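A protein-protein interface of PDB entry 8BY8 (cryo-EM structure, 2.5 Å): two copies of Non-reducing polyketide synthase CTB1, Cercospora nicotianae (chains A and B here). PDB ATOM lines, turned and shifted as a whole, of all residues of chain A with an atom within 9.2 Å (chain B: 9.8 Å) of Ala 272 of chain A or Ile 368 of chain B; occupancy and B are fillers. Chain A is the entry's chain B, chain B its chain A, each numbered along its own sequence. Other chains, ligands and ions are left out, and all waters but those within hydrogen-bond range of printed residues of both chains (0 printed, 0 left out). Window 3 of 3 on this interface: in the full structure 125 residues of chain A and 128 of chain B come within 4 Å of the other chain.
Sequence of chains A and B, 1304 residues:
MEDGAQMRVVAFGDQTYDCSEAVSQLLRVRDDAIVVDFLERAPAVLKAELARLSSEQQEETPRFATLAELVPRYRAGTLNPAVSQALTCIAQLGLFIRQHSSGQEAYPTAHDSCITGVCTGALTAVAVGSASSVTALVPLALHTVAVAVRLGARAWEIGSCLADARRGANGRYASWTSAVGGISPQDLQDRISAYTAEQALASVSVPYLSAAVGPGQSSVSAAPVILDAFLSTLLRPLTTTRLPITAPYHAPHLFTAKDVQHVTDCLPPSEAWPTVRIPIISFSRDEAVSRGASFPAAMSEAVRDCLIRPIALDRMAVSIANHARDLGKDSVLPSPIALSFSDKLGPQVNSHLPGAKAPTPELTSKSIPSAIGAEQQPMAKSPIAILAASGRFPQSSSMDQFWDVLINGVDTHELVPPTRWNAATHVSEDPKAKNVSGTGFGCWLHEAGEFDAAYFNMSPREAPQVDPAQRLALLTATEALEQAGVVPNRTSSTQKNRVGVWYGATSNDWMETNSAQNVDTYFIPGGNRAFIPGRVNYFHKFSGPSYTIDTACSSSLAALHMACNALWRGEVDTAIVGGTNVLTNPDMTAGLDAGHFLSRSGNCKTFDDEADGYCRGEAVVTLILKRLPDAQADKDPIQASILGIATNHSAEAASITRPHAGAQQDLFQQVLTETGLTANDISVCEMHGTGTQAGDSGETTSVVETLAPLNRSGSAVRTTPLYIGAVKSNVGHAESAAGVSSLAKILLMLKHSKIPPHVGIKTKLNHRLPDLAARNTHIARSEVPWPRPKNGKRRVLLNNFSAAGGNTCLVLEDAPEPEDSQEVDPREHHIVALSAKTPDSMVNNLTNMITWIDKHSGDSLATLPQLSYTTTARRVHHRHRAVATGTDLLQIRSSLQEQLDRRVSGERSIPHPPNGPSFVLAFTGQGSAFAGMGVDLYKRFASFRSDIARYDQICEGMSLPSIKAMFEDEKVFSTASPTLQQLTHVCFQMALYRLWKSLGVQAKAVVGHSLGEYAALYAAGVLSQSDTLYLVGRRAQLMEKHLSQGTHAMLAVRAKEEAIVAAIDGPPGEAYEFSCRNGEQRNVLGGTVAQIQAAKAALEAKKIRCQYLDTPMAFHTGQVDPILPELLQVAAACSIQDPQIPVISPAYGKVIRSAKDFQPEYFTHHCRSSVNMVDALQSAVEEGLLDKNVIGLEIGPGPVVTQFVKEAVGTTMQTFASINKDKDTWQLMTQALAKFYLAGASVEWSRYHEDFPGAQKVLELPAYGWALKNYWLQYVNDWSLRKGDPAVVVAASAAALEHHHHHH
The backbone carbonyl oxygen (O) of Pro 369 of chain B is in hydrogen-bond range of a ring nitrogen (NE2) of His 143 of chain A (3.0 Å).
The backbone carbonyl oxygen of Leu 363 of chain B is in hydrogen-bond range of the side-chain hydroxyl of Ser 367 of chain B. The backbone carbonyl oxygen (O) of Thr 364 of chain B lies within hydrogen-bond range of the side-chain hydroxyl (OG) of Ser 367 of chain B. The indole nitrogen (NE1) of Trp 273 of chain A lies within hydrogen-bond range of the backbone carbonyl oxygen (O) of Pro 268 of chain A, at 2.9 Å. The backbone NH of Ala 272 of chain A is in hydrogen-bond range of the side-chain hydroxyl of Ser 270 of chain A (3.0 Å).
Among the printed residues, merely in contact across the chains: Ala 272 of chain A with Ile 368 of chain B, His 143 of chain A with Ala 371 of chain B, Ala 272 of chain A with Ser 367 of chain B, Leu 142 of chain A with Ala 374 of chain B, His 143 of chain A with Ile 368 of chain B, Thr 135 of chain A with Gln 104 of chain B, Trp 273 of chain A with Ile 368 of chain B, His 143 of chain A with Ser 370 of chain B, Ala 136 of chain A with Gln 104 of chain B and Pro 268 of chain A with Pro 369 of chain B.
Ala 141 of chain A touches none of the printed residues of chain B. Printed residues of chain B within 4 Å of Leu 142 of chain A: Ala 374 (3.6 Å). Of the printed residues of chain B, His 143 of chain A touches Ile 368 (3.7 Å), Pro 369 (3.0 Å), Ser 370 (3.9 Å) and Ala 371 (3.3 Å). Printed residues of chain B within 4 Å of Pro 268 of chain A: Pro 369 (3.9 Å). No residue of chain B comes within 4 Å of Ser 270 of chain A. No residue of chain B comes within 4 Å of Glu 271 of chain A. Of chain B, only Ser 367 and Ile 368 come within 4 Å of Ala 272 of chain A. Of chain B, only Ile 368 (3.8 Å) comes within 4 Å of Trp 273 of chain A. Pro 274 of chain A touches none of the printed residues of chain B. No residue of chain A comes within 4 Å of Lys 366 of chain B. Ser 367 of chain B touches one residue of chain A. Ile 368 of chain B touches three residues of chain A. Printed residues of chain A within 4 Å of Pro 369 of chain B: His 143 (3.0 Å) and Pro 268 (3.9 Å). The nearest printed residue of chain A that does not touch Ser 370 of chain B is Pro 139 of chain A (5.8 Å).
Printed residues of chain A that touch a printed residue of chain B: Thr 135, Ala 136, Leu 142, His 143, Pro 268, Ala 272 and Trp 273. Hydrophobic or aromatic side chains of chain A that line the printed part of chain B: Leu 142, His 143, Pro 268 and Ala 272. Of the 13 printed residues of chain B, 7 touch a printed residue of chain A. Along chain B the printed residues that touch a printed residue of chain A span positions 104 to 374. Among the printed residues, 11 pairs touch across the chains.
No position is printed for both chains.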
ATOM      1  N   SER A 130       9.114  -9.810 -21.285  1.00  0.00           N
ATOM      2  CA  SER A 130       9.874  -9.297 -22.416  1.00  0.00           C
ATOM      3  C   SER A 130      11.244  -8.778 -21.990  1.00  0.00           C
ATOM      4  O   SER A 130      11.795  -7.871 -22.617  1.00  0.00           O
ATOM      5  CB  SER A 130       9.090  -8.195 -23.125  1.00  0.00           C
ATOM      6  OG  SER A 130       7.886  -8.700 -23.673  1.00  0.00           O
ATOM      7  N   THR A 135      17.922  -4.488 -15.584  1.00  0.00           N
ATOM      8  CA  THR A 135      18.330  -3.426 -16.496  1.00  0.00           C
ATOM      9  C   THR A 135      17.567  -3.516 -17.811  1.00  0.00           C
ATOM     10  O   THR A 135      17.147  -2.492 -18.363  1.00  0.00           O
ATOM     11  CB  THR A 135      19.839  -3.493 -16.743  1.00  0.00           C
ATOM     12  OG1 THR A 135      20.227  -4.849 -17.001  1.00  0.00           O
ATOM     13  CG2 THR A 135      20.609  -2.965 -15.541  1.00  0.00           C
ATOM     14  N   ALA A 136      17.373  -4.731 -18.325  1.00  0.00           N
ATOM     15  CA  ALA A 136      16.564  -4.925 -19.521  1.00  0.00           C
ATOM     16  C   ALA A 136      15.079  -4.708 -19.266  1.00  0.00           C
ATOM     17  O   ALA A 136      14.304  -4.661 -20.228  1.00  0.00           O
ATOM     18  CB  ALA A 136      16.792  -6.330 -20.080  1.00  0.00           C
ATOM     19  N   LEU A 137      14.667  -4.572 -18.006  1.00  0.00           N
ATOM     20  CA  LEU A 137      13.264  -4.414 -17.648  1.00  0.00           C
ATOM     21  C   LEU A 137      12.857  -2.966 -17.425  1.00  0.00           C
ATOM     22  O   LEU A 137      11.720  -2.605 -17.738  1.00  0.00           O
ATOM     23  CB  LEU A 137      12.955  -5.213 -16.375  1.00  0.00           C
ATOM     24  CG  LEU A 137      11.525  -5.154 -15.828  1.00  0.00           C
ATOM     25  CD1 LEU A 137      10.648  -6.197 -16.490  1.00  0.00           C
ATOM     26  CD2 LEU A 137      11.531  -5.330 -14.321  1.00  0.00           C
ATOM     27  N   VAL A 138      13.750  -2.131 -16.892  1.00  0.00           N
ATOM     28  CA  VAL A 138      13.350  -0.776 -16.501  1.00  0.00           C
ATOM     29  C   VAL A 138      12.695  -0.006 -17.646  1.00  0.00           C
ATOM     30  O   VAL A 138      11.618   0.578 -17.433  1.00  0.00           O
ATOM     31  CB  VAL A 138      14.555  -0.023 -15.908  1.00  0.00           C
ATOM     32  CG1 VAL A 138      14.200   1.430 -15.646  1.00  0.00           C
ATOM     33  CG2 VAL A 138      15.019  -0.701 -14.631  1.00  0.00           C
ATOM     34  N   PRO A 139      13.271   0.056 -18.852  1.00  0.00           N
ATOM     35  CA  PRO A 139      12.608   0.828 -19.920  1.00  0.00           C
ATOM     36  C   PRO A 139      11.250   0.272 -20.316  1.00  0.00           C
ATOM     37  O   PRO A 139      10.301   1.042 -20.528  1.00  0.00           O
ATOM     38  CB  PRO A 139      13.620   0.766 -21.075  1.00  0.00           C
ATOM     39  CG  PRO A 139      14.493  -0.401 -20.772  1.00  0.00           C
ATOM     40  CD  PRO A 139      14.573  -0.479 -19.286  1.00  0.00           C
ATOM     41  N   LEU A 140      11.130  -1.053 -20.435  1.00  0.00           N
ATOM     42  CA  LEU A 140       9.821  -1.646 -20.678  1.00  0.00           C
ATOM     43  C   LEU A 140       8.861  -1.319 -19.543  1.00  0.00           C
ATOM     44  O   LEU A 140       7.661  -1.131 -19.770  1.00  0.00           O
ATOM     45  CB  LEU A 140       9.952  -3.158 -20.853  1.00  0.00           C
ATOM     46  CG  LEU A 140      10.894  -3.638 -21.959  1.00  0.00           C
ATOM     47  CD1 LEU A 140      10.727  -5.127 -22.182  1.00  0.00           C
ATOM     48  CD2 LEU A 140      10.663  -2.884 -23.252  1.00  0.00           C
ATOM     49  N   ALA A 141       9.371  -1.242 -18.312  1.00  0.00           N
ATOM     50  CA  ALA A 141       8.522  -0.873 -17.186  1.00  0.00           C
ATOM     51  C   ALA A 141       7.982   0.542 -17.342  1.00  0.00           C
ATOM     52  O   ALA A 141       6.811   0.803 -17.047  1.00  0.00           O
ATOM     53  CB  ALA A 141       9.300  -1.013 -15.878  1.00  0.00           C
ATOM     54  N   LEU A 142       8.820   1.475 -17.798  1.00  0.00           N
ATOM     55  CA  LEU A 142       8.340   2.841 -18.008  1.00  0.00           C
ATOM     56  C   LEU A 142       7.320   2.903 -19.145  1.00  0.00           C
ATOM     57  O   LEU A 142       6.301   3.609 -19.046  1.00  0.00           O
ATOM     58  CB  LEU A 142       9.526   3.763 -18.280  1.00  0.00           C
ATOM     59  CG  LEU A 142      10.506   3.874 -17.110  1.00  0.00           C
ATOM     60  CD1 LEU A 142      11.881   4.270 -17.602  1.00  0.00           C
ATOM     61  CD2 LEU A 142       9.998   4.875 -16.088  1.00  0.00           C
ATOM     62  N   HIS A 143       7.573   2.162 -20.227  1.00  0.00           N
ATOM     63  CA  HIS A 143       6.583   2.067 -21.296  1.00  0.00           C
ATOM     64  C   HIS A 143       5.251   1.557 -20.757  1.00  0.00           C
ATOM     65  O   HIS A 143       4.182   2.078 -21.106  1.00  0.00           O
ATOM     66  CB  HIS A 143       7.091   1.144 -22.406  1.00  0.00           C
ATOM     67  CG  HIS A 143       8.081   1.787 -23.329  1.00  0.00           C
ATOM     68  ND1 HIS A 143       8.151   3.150 -23.516  1.00  0.00           N
ATOM     69  CD2 HIS A 143       9.036   1.249 -24.123  1.00  0.00           C
ATOM     70  CE1 HIS A 143       9.109   3.425 -24.382  1.00  0.00           C
ATOM     71  NE2 HIS A 143       9.662   2.289 -24.767  1.00  0.00           N
ATOM     72  N   LEU A 267       3.578   3.667 -27.919  1.00  0.00           N
ATOM     73  CA  LEU A 267       4.769   2.885 -28.205  1.00  0.00           C
ATOM     74  C   LEU A 267       5.187   3.139 -29.645  1.00  0.00           C
ATOM     75  O   LEU A 267       4.515   2.649 -30.566  1.00  0.00           O
ATOM     76  CB  LEU A 267       4.500   1.398 -27.985  1.00  0.00           C
ATOM     77  CG  LEU A 267       3.792   1.031 -26.679  1.00  0.00           C
ATOM     78  CD1 LEU A 267       3.561  -0.466 -26.600  1.00  0.00           C
ATOM     79  CD2 LEU A 267       4.581   1.508 -25.474  1.00  0.00           C
ATOM     80  N   PRO A 268       6.268   3.874 -29.898  1.00  0.00           N
ATOM     81  CA  PRO A 268       6.661   4.124 -31.280  1.00  0.00           C
ATOM     82  C   PRO A 268       6.982   2.826 -31.984  1.00  0.00           C
ATOM     83  O   PRO A 268       7.474   1.864 -31.363  1.00  0.00           O
ATOM     84  CB  PRO A 268       7.905   5.012 -31.137  1.00  0.00           C
ATOM     85  CG  PRO A 268       7.787   5.627 -29.794  1.00  0.00           C
ATOM     86  CD  PRO A 268       7.126   4.595 -28.944  1.00  0.00           C
ATOM     87  N   PRO A 269       6.718   2.739 -33.288  1.00  0.00           N
ATOM     88  CA  PRO A 269       7.008   1.500 -34.012  1.00  0.00           C
ATOM     89  C   PRO A 269       8.499   1.311 -34.232  1.00  0.00           C
ATOM     90  O   PRO A 269       9.264   2.268 -34.368  1.00  0.00           O
ATOM     91  CB  PRO A 269       6.272   1.681 -35.347  1.00  0.00           C
ATOM     92  CG  PRO A 269       5.648   3.057 -35.310  1.00  0.00           C
ATOM     93  CD  PRO A 269       6.292   3.810 -34.203  1.00  0.00           C
ATOM     94  N   SER A 270       8.904   0.044 -34.268  1.00  0.00           N
ATOM     95  CA  SER A 270      10.295  -0.314 -34.506  1.00  0.00           C
ATOM     96  C   SER A 270      10.399  -1.830 -34.563  1.00  0.00           C
ATOM     97  O   SER A 270       9.494  -2.547 -34.127  1.00  0.00           O
ATOM     98  CB  SER A 270      11.220   0.242 -33.418  1.00  0.00           C
ATOM     99  OG  SER A 270      12.540  -0.246 -33.581  1.00  0.00           O
ATOM    100  N   GLU A 271      11.517  -2.309 -35.109  1.00  0.00           N
ATOM    101  CA  GLU A 271      11.843  -3.728 -35.115  1.00  0.00           C
ATOM    102  C   GLU A 271      12.758  -4.106 -33.953  1.00  0.00           C
ATOM    103  O   GLU A 271      13.136  -5.273 -33.818  1.00  0.00           O
ATOM    104  CB  GLU A 271      12.483  -4.111 -36.452  1.00  0.00           C
ATOM    105  CG  GLU A 271      12.891  -5.574 -36.572  1.00  0.00           C
ATOM    106  CD  GLU A 271      11.792  -6.527 -36.145  1.00  0.00           C
ATOM    107  OE1 GLU A 271      10.657  -6.391 -36.647  1.00  0.00           O
ATOM    108  OE2 GLU A 271      12.061  -7.404 -35.297  1.00  0.00           O
ATOM    109  N   ALA A 272      13.089  -3.144 -33.095  1.00  0.00           N
ATOM    110  CA  ALA A 272      13.951  -3.379 -31.947  1.00  0.00           C
ATOM    111  C   ALA A 272      13.185  -3.843 -30.717  1.00  0.00           C
ATOM    112  O   ALA A 272      13.808  -4.121 -29.688  1.00  0.00           O
ATOM    113  CB  ALA A 272      14.727  -2.105 -31.603  1.00  0.00           C
ATOM    114  N   TRP A 273      11.864  -3.937 -30.793  1.00  0.00           N
ATOM    115  CA  TRP A 273      11.084  -4.341 -29.631  1.00  0.00           C
ATOM    116  C   TRP A 273      11.402  -5.789 -29.272  1.00  0.00           C
ATOM    117  O   TRP A 273      11.385  -6.658 -30.151  1.00  0.00           O
ATOM    118  CB  TRP A 273       9.591  -4.187 -29.906  1.00  0.00           C
ATOM    119  CG  TRP A 273       9.147  -2.765 -30.012  1.00  0.00           C
ATOM    120  CD1 TRP A 273       8.699  -2.130 -31.128  1.00  0.00           C
ATOM    121  CD2 TRP A 273       9.115  -1.796 -28.957  1.00  0.00           C
ATOM    122  NE1 TRP A 273       8.386  -0.825 -30.838  1.00  0.00           N
ATOM    123  CE2 TRP A 273       8.633  -0.595 -29.511  1.00  0.00           C
ATOM    124  CE3 TRP A 273       9.445  -1.828 -27.600  1.00  0.00           C
ATOM    125  CZ2 TRP A 273       8.474   0.563 -28.756  1.00  0.00           C
ATOM    126  CZ3 TRP A 273       9.286  -0.677 -26.853  1.00  0.00           C
ATOM    127  CH2 TRP A 273       8.805   0.502 -27.432  1.00  0.00           C
ATOM    128  N   PRO A 274      11.704  -6.089 -28.010  1.00  0.00           N
ATOM    129  CA  PRO A 274      11.911  -7.486 -27.625  1.00  0.00           C
ATOM    130  C   PRO A 274      10.610  -8.267 -27.664  1.00  0.00           C
ATOM    131  O   PRO A 274       9.521  -7.714 -27.496  1.00  0.00           O
ATOM    132  CB  PRO A 274      12.458  -7.383 -26.198  1.00  0.00           C
ATOM    133  CG  PRO A 274      11.910  -6.105 -25.687  1.00  0.00           C
ATOM    134  CD  PRO A 274      11.854  -5.177 -26.863  1.00  0.00           C
ATOM    135  N   THR A 275      10.733  -9.569 -27.892  1.00  0.00           N
ATOM    136  CA  THR A 275       9.580 -10.454 -27.903  1.00  0.00           C
ATOM    137  C   THR A 275       9.269 -10.897 -26.475  1.00  0.00           C
ATOM    138  O   THR A 275       9.813 -10.368 -25.502  1.00  0.00           O
ATOM    139  CB  THR A 275       9.834 -11.649 -28.819  1.00  0.00           C
ATOM    140  OG1 THR A 275      10.912 -12.436 -28.298  1.00  0.00           O
ATOM    141  CG2 THR A 275      10.183 -11.181 -30.218  1.00  0.00           C
ATOM    142  N   SER A 294       5.427  -9.926 -29.960  1.00  0.00           N
ATOM    143  CA  SER A 294       6.285  -8.784 -29.698  1.00  0.00           C
ATOM    144  C   SER A 294       5.758  -7.989 -28.505  1.00  0.00           C
ATOM    145  O   SER A 294       4.647  -8.209 -28.019  1.00  0.00           O
ATOM    146  CB  SER A 294       6.375  -7.895 -30.934  1.00  0.00           C
ATOM    147  OG  SER A 294       7.192  -6.766 -30.685  1.00  0.00           O
ATOM    148  N   PHE A 295       6.576  -7.052 -28.030  1.00  0.00           N
ATOM    149  CA  PHE A 295       6.174  -6.254 -26.872  1.00  0.00           C
ATOM    150  C   PHE A 295       4.925  -5.428 -27.144  1.00  0.00           C
ATOM    151  O   PHE A 295       3.983  -5.489 -26.333  1.00  0.00           O
ATOM    152  CB  PHE A 295       7.345  -5.372 -26.426  1.00  0.00           C
ATOM    153  CG  PHE A 295       7.043  -4.518 -25.229  1.00  0.00           C
ATOM    154  CD1 PHE A 295       7.021  -5.063 -23.959  1.00  0.00           C
ATOM    155  CD2 PHE A 295       6.792  -3.165 -25.373  1.00  0.00           C
ATOM    156  CE1 PHE A 295       6.748  -4.277 -22.859  1.00  0.00           C
ATOM    157  CE2 PHE A 295       6.519  -2.377 -24.273  1.00  0.00           C
ATOM    158  CZ  PHE A 295       6.499  -2.935 -23.018  1.00  0.00           C
ATOM    159  N   PRO A 296       4.822  -4.665 -28.244  1.00  0.00           N
ATOM    160  CA  PRO A 296       3.622  -3.841 -28.446  1.00  0.00           C
ATOM    161  C   PRO A 296       2.398  -4.669 -28.801  1.00  0.00           C
ATOM    162  O   PRO A 296       1.279  -4.336 -28.400  1.00  0.00           O
ATOM    163  CB  PRO A 296       4.022  -2.907 -29.600  1.00  0.00           C
ATOM    164  CG  PRO A 296       5.502  -3.085 -29.779  1.00  0.00           C
ATOM    165  CD  PRO A 296       5.789  -4.476 -29.335  1.00  0.00           C
ATOM    166  N   SER B 102      24.363  -0.605 -19.629  1.00  0.00           N
ATOM    167  CA  SER B 102      23.882   0.419 -20.548  1.00  0.00           C
ATOM    168  C   SER B 102      23.900  -0.062 -21.992  1.00  0.00           C
ATOM    169  O   SER B 102      23.066   0.369 -22.794  1.00  0.00           O
ATOM    170  CB  SER B 102      24.724   1.686 -20.405  1.00  0.00           C
ATOM    171  OG  SER B 102      24.322   2.671 -21.337  1.00  0.00           O
ATOM    172  N   GLN B 104      23.150  -2.994 -23.081  1.00  0.00           N
ATOM    173  CA  GLN B 104      22.115  -3.992 -23.332  1.00  0.00           C
ATOM    174  C   GLN B 104      22.711  -5.262 -23.936  1.00  0.00           C
ATOM    175  O   GLN B 104      22.203  -5.817 -24.913  1.00  0.00           O
ATOM    176  CB  GLN B 104      21.019  -3.418 -24.231  1.00  0.00           C
ATOM    177  CG  GLN B 104      20.220  -2.283 -23.596  1.00  0.00           C
ATOM    178  CD  GLN B 104      19.324  -2.751 -22.459  1.00  0.00           C
ATOM    179  OE1 GLN B 104      19.327  -2.173 -21.372  1.00  0.00           O
ATOM    180  NE2 GLN B 104      18.542  -3.796 -22.714  1.00  0.00           N
ATOM    181  N   LEU B 363      24.459  -2.443 -34.400  1.00  0.00           N
ATOM    182  CA  LEU B 363      23.982  -2.141 -33.056  1.00  0.00           C
ATOM    183  C   LEU B 363      22.463  -2.081 -32.965  1.00  0.00           C
ATOM    184  O   LEU B 363      21.926  -2.027 -31.853  1.00  0.00           O
ATOM    185  CB  LEU B 363      24.581  -0.810 -32.583  1.00  0.00           C
ATOM    186  CG  LEU B 363      24.933  -0.639 -31.101  1.00  0.00           C
ATOM    187  CD1 LEU B 363      25.795   0.598 -30.896  1.00  0.00           C
ATOM    188  CD2 LEU B 363      23.688  -0.568 -30.229  1.00  0.00           C
ATOM    189  N   THR B 364      21.762  -2.102 -34.100  1.00  0.00           N
ATOM    190  CA  THR B 364      20.298  -2.075 -34.130  1.00  0.00           C
ATOM    191  C   THR B 364      19.753  -0.739 -33.621  1.00  0.00           C
ATOM    192  O   THR B 364      18.896  -0.689 -32.737  1.00  0.00           O
ATOM    193  CB  THR B 364      19.709  -3.242 -33.331  1.00  0.00           C
ATOM    194  OG1 THR B 364      20.306  -4.471 -33.766  1.00  0.00           O
ATOM    195  CG2 THR B 364      18.205  -3.318 -33.539  1.00  0.00           C
ATOM    196  N   SER B 365      20.261   0.350 -34.189  1.00  0.00           N
ATOM    197  CA  SER B 365      19.754   1.694 -33.881  1.00  0.00           C
ATOM    198  C   SER B 365      19.911   1.923 -32.375  1.00  0.00           C
ATOM    199  O   SER B 365      20.797   1.339 -31.737  1.00  0.00           O
ATOM    200  CB  SER B 365      18.335   1.833 -34.402  1.00  0.00           C
ATOM    201  OG  SER B 365      18.260   1.479 -35.772  1.00  0.00           O
ATOM    202  N   LYS B 366      19.064   2.773 -31.791  1.00  0.00           N
ATOM    203  CA  LYS B 366      19.068   2.948 -30.344  1.00  0.00           C
ATOM    204  C   LYS B 366      18.430   1.770 -29.619  1.00  0.00           C
ATOM    205  O   LYS B 366      18.459   1.736 -28.385  1.00  0.00           O
ATOM    206  CB  LYS B 366      18.353   4.247 -29.964  1.00  0.00           C
ATOM    207  CG  LYS B 366      16.845   4.215 -30.135  1.00  0.00           C
ATOM    208  CD  LYS B 366      16.252   5.621 -30.210  1.00  0.00           C
ATOM    209  CE  LYS B 366      16.701   6.516 -29.056  1.00  0.00           C
ATOM    210  NZ  LYS B 366      16.400   5.947 -27.711  1.00  0.00           N
ATOM    211  N   SER B 367      17.860   0.815 -30.352  1.00  0.00           N
ATOM    212  CA  SER B 367      17.279  -0.394 -29.773  1.00  0.00           C
ATOM    213  C   SER B 367      16.108  -0.050 -28.850  1.00  0.00           C
ATOM    214  O   SER B 367      16.138  -0.291 -27.645  1.00  0.00           O
ATOM    215  CB  SER B 367      18.350  -1.208 -29.038  1.00  0.00           C
ATOM    216  OG  SER B 367      19.417  -1.536 -29.910  1.00  0.00           O
ATOM    217  N   ILE B 368      15.080   0.540 -29.461  1.00  0.00           N
ATOM    218  CA  ILE B 368      13.801   0.942 -28.864  1.00  0.00           C
ATOM    219  C   ILE B 368      13.949   2.349 -28.292  1.00  0.00           C
ATOM    220  O   ILE B 368      14.999   2.670 -27.716  1.00  0.00           O
ATOM    221  CB  ILE B 368      13.275  -0.056 -27.806  1.00  0.00           C
ATOM    222  CG1 ILE B 368      13.889   0.150 -26.405  1.00  0.00           C
ATOM    223  CG2 ILE B 368      13.431  -1.503 -28.287  1.00  0.00           C
ATOM    224  CD1 ILE B 368      12.878   0.526 -25.345  1.00  0.00           C
ATOM    225  N   PRO B 369      12.956   3.223 -28.439  1.00  0.00           N
ATOM    226  CA  PRO B 369      13.064   4.566 -27.865  1.00  0.00           C
ATOM    227  C   PRO B 369      12.664   4.580 -26.395  1.00  0.00           C
ATOM    228  O   PRO B 369      12.024   3.663 -25.882  1.00  0.00           O
ATOM    229  CB  PRO B 369      12.092   5.404 -28.709  1.00  0.00           C
ATOM    230  CG  PRO B 369      11.567   4.483 -29.780  1.00  0.00           C
ATOM    231  CD  PRO B 369      11.748   3.100 -29.269  1.00  0.00           C
ATOM    232  N   SER B 370      13.047   5.660 -25.723  1.00  0.00           N
ATOM    233  CA  SER B 370      12.724   5.853 -24.316  1.00  0.00           C
ATOM    234  C   SER B 370      11.391   6.578 -24.191  1.00  0.00           C
ATOM    235  O   SER B 370      11.100   7.495 -24.965  1.00  0.00           O
ATOM    236  CB  SER B 370      13.825   6.646 -23.610  1.00  0.00           C
ATOM    237  OG  SER B 370      14.993   5.863 -23.443  1.00  0.00           O
ATOM    238  N   ALA B 371      10.582   6.154 -23.224  1.00  0.00           N
ATOM    239  CA  ALA B 371       9.295   6.792 -22.990  1.00  0.00           C
ATOM    240  C   ALA B 371       9.490   8.264 -22.660  1.00  0.00           C
ATOM    241  O   ALA B 371      10.467   8.646 -22.010  1.00  0.00           O
ATOM    242  CB  ALA B 371       8.557   6.088 -21.851  1.00  0.00           C
ATOM    243  N   ALA B 374      11.488   9.716 -19.812  1.00  0.00           N
ATOM    244  CA  ALA B 374      12.550   8.785 -19.456  1.00  0.00           C
ATOM    245  C   ALA B 374      13.775   8.920 -20.348  1.00  0.00           C
ATOM    246  O   ALA B 374      14.758   8.200 -20.144  1.00  0.00           O
ATOM    247  CB  ALA B 374      12.031   7.347 -19.518  1.00  0.00           C
ATOM    248  N   GLU B 375      13.741   9.821 -21.329  1.00  0.00           N
ATOM    249  CA  GLU B 375      14.874  10.040 -22.218  1.00  0.00           C
ATOM    250  C   GLU B 375      15.939  10.932 -21.598  1.00  0.00           C
ATOM    251  O   GLU B 375      17.031  11.050 -22.161  1.00  0.00           O
ATOM    252  CB  GLU B 375      14.396  10.670 -23.530  1.00  0.00           C
ATOM    253  CG  GLU B 375      13.211   9.968 -24.182  1.00  0.00           C
ATOM    254  CD  GLU B 375      12.229  10.943 -24.800  1.00  0.00           C
ATOM    255  OE1 GLU B 375      12.117  10.972 -26.043  1.00  0.00           O
ATOM    256  OE2 GLU B 375      11.578  11.689 -24.041  1.00  0.00           O
